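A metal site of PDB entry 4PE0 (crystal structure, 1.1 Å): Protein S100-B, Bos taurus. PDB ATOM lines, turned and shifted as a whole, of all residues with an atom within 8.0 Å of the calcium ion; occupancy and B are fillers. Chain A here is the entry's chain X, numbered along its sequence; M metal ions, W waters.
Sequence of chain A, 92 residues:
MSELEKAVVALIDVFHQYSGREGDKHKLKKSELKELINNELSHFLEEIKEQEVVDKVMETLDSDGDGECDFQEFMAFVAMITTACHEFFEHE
The calcium ion is bound by the side-chain carboxylate (OD1) of Asp 62, the side-chain carboxylate (OD2) of Asp 64, the backbone carbonyl oxygen (O) of Glu 68, the side-chain carboxylate (OD1) of Asp 66, water W1, the side-chain carboxylate (OE1) of Glu 73 and the side-chain carboxylate (OE2) of Glu 73.
OD2 of Asp 66 is in salt-bridge range of NZ of Lys 27, 3.0 Å away. The side-chain carboxylate (OE2) of Glu 73 lies close to the backbone NH (N) of Ser 63. N of Gly 65 lies close to OD1 of Asp 62, 3.0 Å away. The side-chain carboxylate (OD1) of Asp 70 is in hydrogen-bond range of the backbone NH (N) of Glu 73 (2.9 Å). The backbone NH (N) of Gly 67 sits at hydrogen-bond distance from the side-chain carboxylate (OD2) of Asp 62 (2.9 Å).
Of the 17 residues printed, 5 come within 4 Å of the calcium ion.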
ATOM      1  N   LYS A  27      32.919  -7.555  27.081  1.00  0.00           N
ATOM      2  CA  LYS A  27      31.834  -8.458  26.728  1.00  0.00           C
ATOM      3  C   LYS A  27      32.208  -9.234  25.502  1.00  0.00           C
ATOM      4  O   LYS A  27      32.956  -8.730  24.661  1.00  0.00           O
ATOM      5  CB  LYS A  27      30.558  -7.689  26.419  1.00  0.00           C
ATOM      6  CG  LYS A  27      30.064  -6.836  27.561  1.00  0.00           C
ATOM      7  CD  LYS A  27      28.898  -5.982  27.105  1.00  0.00           C
ATOM      8  CE  LYS A  27      28.473  -5.008  28.184  1.00  0.00           C
ATOM      9  NZ  LYS A  27      27.454  -4.053  27.674  1.00  0.00           N
ATOM     10  N   LEU A  28      31.662 -10.454  25.405  1.00  0.00           N
ATOM     11  CA  LEU A  28      31.791 -11.279  24.203  1.00  0.00           C
ATOM     12  C   LEU A  28      30.626 -11.004  23.272  1.00  0.00           C
ATOM     13  O   LEU A  28      29.490 -11.245  23.623  1.00  0.00           O
ATOM     14  CB  LEU A  28      31.746 -12.752  24.566  1.00  0.00           C
ATOM     15  CG  LEU A  28      32.830 -13.259  25.496  1.00  0.00           C
ATOM     16  CD1 LEU A  28      32.456 -14.605  26.105  1.00  0.00           C
ATOM     17  CD2 LEU A  28      34.154 -13.395  24.796  1.00  0.00           C
ATOM     18  N   MET A  58      24.052 -17.628  22.222  1.00  0.00           N
ATOM     19  CA  MET A  58      24.054 -16.297  22.810  1.00  0.00           C
ATOM     20  C   MET A  58      22.717 -16.005  23.474  1.00  0.00           C
ATOM     21  O   MET A  58      22.691 -15.447  24.575  1.00  0.00           O
ATOM     22  CB  MET A  58      24.379 -15.224  21.777  1.00  0.00           C
ATOM     23  CG  MET A  58      24.389 -13.828  22.399  1.00  0.00           C
ATOM     24  SD  MET A  58      25.707 -13.572  23.585  1.00  0.00           S
ATOM     25  CE  MET A  58      27.084 -13.262  22.463  1.00  0.00           C
ATOM     26  N   LEU A  61      22.712 -17.610  26.858  1.00  0.00           N
ATOM     27  CA  LEU A  61      23.657 -17.066  27.836  1.00  0.00           C
ATOM     28  C   LEU A  61      23.396 -15.625  28.239  1.00  0.00           C
ATOM     29  O   LEU A  61      23.772 -15.217  29.339  1.00  0.00           O
ATOM     30  CB  LEU A  61      25.095 -17.180  27.315  1.00  0.00           C
ATOM     31  CG  LEU A  61      25.600 -18.594  27.057  1.00  0.00           C
ATOM     32  CD1 LEU A  61      27.058 -18.585  26.633  1.00  0.00           C
ATOM     33  CD2 LEU A  61      25.424 -19.489  28.279  1.00  0.00           C
ATOM     34  N   ASP A  62      22.722 -14.882  27.359  1.00  0.00           N
ATOM     35  CA  ASP A  62      22.550 -13.450  27.535  1.00  0.00           C
ATOM     36  C   ASP A  62      21.355 -13.146  28.444  1.00  0.00           C
ATOM     37  O   ASP A  62      20.290 -12.734  27.984  1.00  0.00           O
ATOM     38  CB  ASP A  62      22.391 -12.760  26.169  1.00  0.00           C
ATOM     39  CG  ASP A  62      22.144 -11.258  26.296  1.00  0.00           C
ATOM     40  OD1 ASP A  62      22.598 -10.635  27.270  1.00  0.00           O
ATOM     41  OD2 ASP A  62      21.479 -10.690  25.387  1.00  0.00           O
ATOM     42  N   SER A  63      21.570 -13.293  29.747  1.00  0.00           N
ATOM     43  CA  SER A  63      20.499 -13.084  30.725  1.00  0.00           C
ATOM     44  C   SER A  63      20.080 -11.627  30.870  1.00  0.00           C
ATOM     45  O   SER A  63      18.929 -11.350  31.213  1.00  0.00           O
ATOM     46  CB  SER A  63      20.914 -13.637  32.085  1.00  0.00           C
ATOM     47  OG  SER A  63      21.260 -15.005  32.008  1.00  0.00           O
ATOM     48  N   ASP A  64      20.981 -10.679  30.625  1.00  0.00           N
ATOM     49  CA  ASP A  64      20.626  -9.264  30.846  1.00  0.00           C
ATOM     50  C   ASP A  64      20.220  -8.528  29.557  1.00  0.00           C
ATOM     51  O   ASP A  64      19.979  -7.313  29.589  1.00  0.00           O
ATOM     52  CB  ASP A  64      21.736  -8.516  31.595  1.00  0.00           C
ATOM     53  CG  ASP A  64      23.009  -8.377  30.785  1.00  0.00           C
ATOM     54  OD1 ASP A  64      24.048  -8.071  31.415  1.00  0.00           O
ATOM     55  OD2 ASP A  64      22.971  -8.558  29.546  1.00  0.00           O
ATOM     56  N   GLY A  65      20.157  -9.252  28.449  1.00  0.00           N
ATOM     57  CA  GLY A  65      19.531  -8.769  27.230  1.00  0.00           C
ATOM     58  C   GLY A  65      20.282  -7.736  26.411  1.00  0.00           C
ATOM     59  O   GLY A  65      19.710  -7.156  25.485  1.00  0.00           O
ATOM     60  N   ASP A  66      21.554  -7.508  26.711  1.00  0.00           N
ATOM     61  CA  ASP A  66      22.307  -6.483  25.984  1.00  0.00           C
ATOM     62  C   ASP A  66      22.918  -7.019  24.683  1.00  0.00           C
ATOM     63  O   ASP A  66      23.682  -6.325  24.026  1.00  0.00           O
ATOM     64  CB  ASP A  66      23.367  -5.824  26.873  1.00  0.00           C
ATOM     65  CG  ASP A  66      24.494  -6.759  27.253  1.00  0.00           C
ATOM     66  OD1 ASP A  66      24.420  -7.973  26.913  1.00  0.00           O
ATOM     67  OD2 ASP A  66      25.450  -6.266  27.890  1.00  0.00           O
ATOM     68  N   GLY A  67      22.569  -8.262  24.345  1.00  0.00           N
ATOM     69  CA  GLY A  67      22.994  -8.878  23.097  1.00  0.00           C
ATOM     70  C   GLY A  67      24.364  -9.542  23.121  1.00  0.00           C
ATOM     71  O   GLY A  67      24.817 -10.108  22.118  1.00  0.00           O
ATOM     72  N   GLU A  68      25.010  -9.504  24.276  1.00  0.00           N
ATOM     73  CA  GLU A  68      26.375 -10.017  24.395  1.00  0.00           C
ATOM     74  C   GLU A  68      26.517 -10.782  25.685  1.00  0.00           C
ATOM     75  O   GLU A  68      25.603 -10.789  26.497  1.00  0.00           O
ATOM     76  CB  GLU A  68      27.389  -8.872  24.346  1.00  0.00           C
ATOM     77  CG  GLU A  68      27.315  -8.041  23.064  1.00  0.00           C
ATOM     78  CD  GLU A  68      28.571  -7.231  22.762  1.00  0.00           C
ATOM     79  OE1 GLU A  68      29.661  -7.565  23.277  1.00  0.00           O
ATOM     80  OE2 GLU A  68      28.454  -6.239  22.003  1.00  0.00           O
ATOM     81  N   CYS A  69      27.652 -11.438  25.857  1.00  0.00           N
ATOM     82  CA  CYS A  69      27.907 -12.232  27.047  1.00  0.00           C
ATOM     83  C   CYS A  69      28.957 -11.555  27.910  1.00  0.00           C
ATOM     84  O   CYS A  69      30.101 -11.445  27.519  1.00  0.00           O
ATOM     85  CB  CYS A  69      28.372 -13.627  26.633  1.00  0.00           C
ATOM     86  SG  CYS A  69      28.647 -14.786  27.998  1.00  0.00           S
ATOM     87  N   ASP A  70      28.550 -11.100  29.100  1.00  0.00           N
ATOM     88  CA  ASP A  70      29.478 -10.445  30.012  1.00  0.00           C
ATOM     89  C   ASP A  70      30.112 -11.499  30.931  1.00  0.00           C
ATOM     90  O   ASP A  70      29.848 -12.714  30.775  1.00  0.00           O
ATOM     91  CB  ASP A  70      28.833  -9.290  30.813  1.00  0.00           C
ATOM     92  CG  ASP A  70      27.692  -9.741  31.716  1.00  0.00           C
ATOM     93  OD1 ASP A  70      27.599 -10.949  32.069  1.00  0.00           O
ATOM     94  OD2 ASP A  70      26.899  -8.864  32.133  1.00  0.00           O
ATOM     95  N   PHE A  71      30.956 -11.056  31.857  1.00  0.00           N
ATOM     96  CA  PHE A  71      31.676 -12.016  32.664  1.00  0.00           C
ATOM     97  C   PHE A  71      30.749 -12.875  33.508  1.00  0.00           C
ATOM     98  O   PHE A  71      30.951 -14.090  33.633  1.00  0.00           O
ATOM     99  CB  PHE A  71      32.726 -11.355  33.554  1.00  0.00           C
ATOM    100  CG  PHE A  71      33.627 -12.370  34.197  1.00  0.00           C
ATOM    101  CD1 PHE A  71      34.513 -13.096  33.424  1.00  0.00           C
ATOM    102  CD2 PHE A  71      33.534 -12.681  35.548  1.00  0.00           C
ATOM    103  CE1 PHE A  71      35.329 -14.061  33.973  1.00  0.00           C
ATOM    104  CE2 PHE A  71      34.357 -13.658  36.095  1.00  0.00           C
ATOM    105  CZ  PHE A  71      35.242 -14.342  35.320  1.00  0.00           C
ATOM    106  N   GLN A  72      29.743 -12.255  34.116  1.00  0.00           N
ATOM    107  CA  GLN A  72      28.782 -13.004  34.925  1.00  0.00           C
ATOM    108  C   GLN A  72      28.098 -14.097  34.129  1.00  0.00           C
ATOM    109  O   GLN A  72      27.929 -15.242  34.576  1.00  0.00           O
ATOM    110  CB  GLN A  72      27.734 -12.032  35.502  1.00  0.00           C
ATOM    111  CG  GLN A  72      26.522 -12.676  36.133  1.00  0.00           C
ATOM    112  CD  GLN A  72      25.391 -11.672  36.324  1.00  0.00           C
ATOM    113  OE1 GLN A  72      25.235 -10.737  35.526  1.00  0.00           O
ATOM    114  NE2 GLN A  72      24.600 -11.850  37.374  1.00  0.00           N
ATOM    115  N   GLU A  73      27.710 -13.756  32.906  1.00  0.00           N
ATOM    116  CA  GLU A  73      27.048 -14.694  32.039  1.00  0.00           C
ATOM    117  C   GLU A  73      28.019 -15.777  31.590  1.00  0.00           C
ATOM    118  O   GLU A  73      27.644 -16.947  31.456  1.00  0.00           O
ATOM    119  CB  GLU A  73      26.440 -13.922  30.871  1.00  0.00           C
ATOM    120  CG  GLU A  73      25.322 -12.979  31.304  1.00  0.00           C
ATOM    121  CD  GLU A  73      24.963 -11.918  30.276  1.00  0.00           C
ATOM    122  OE1 GLU A  73      25.751 -11.689  29.340  1.00  0.00           O
ATOM    123  OE2 GLU A  73      23.866 -11.326  30.384  1.00  0.00           O
ATOM    124  N   PHE A  74      29.263 -15.407  31.359  1.00  0.00           N
ATOM    125  CA  PHE A  74      30.305 -16.395  31.037  1.00  0.00           C
ATOM    126  C   PHE A  74      30.529 -17.365  32.201  1.00  0.00           C
ATOM    127  O   PHE A  74      30.670 -18.585  31.992  1.00  0.00           O
ATOM    128  CB  PHE A  74      31.616 -15.694  30.634  1.00  0.00           C
ATOM    129  CG  PHE A  74      32.744 -16.650  30.361  1.00  0.00           C
ATOM    130  CD1 PHE A  74      32.716 -17.441  29.235  1.00  0.00           C
ATOM    131  CD2 PHE A  74      33.821 -16.753  31.216  1.00  0.00           C
ATOM    132  CE1 PHE A  74      33.748 -18.322  28.968  1.00  0.00           C
ATOM    133  CE2 PHE A  74      34.858 -17.641  30.926  1.00  0.00           C
ATOM    134  CZ  PHE A  74      34.806 -18.407  29.808  1.00  0.00           C
HETATM  135 CA    CA M   1      24.476  -9.868  28.356  1.00  0.00          CA
HETATM  136  O   HOH W   1      26.203  -8.435  29.274  1.00  0.00           O
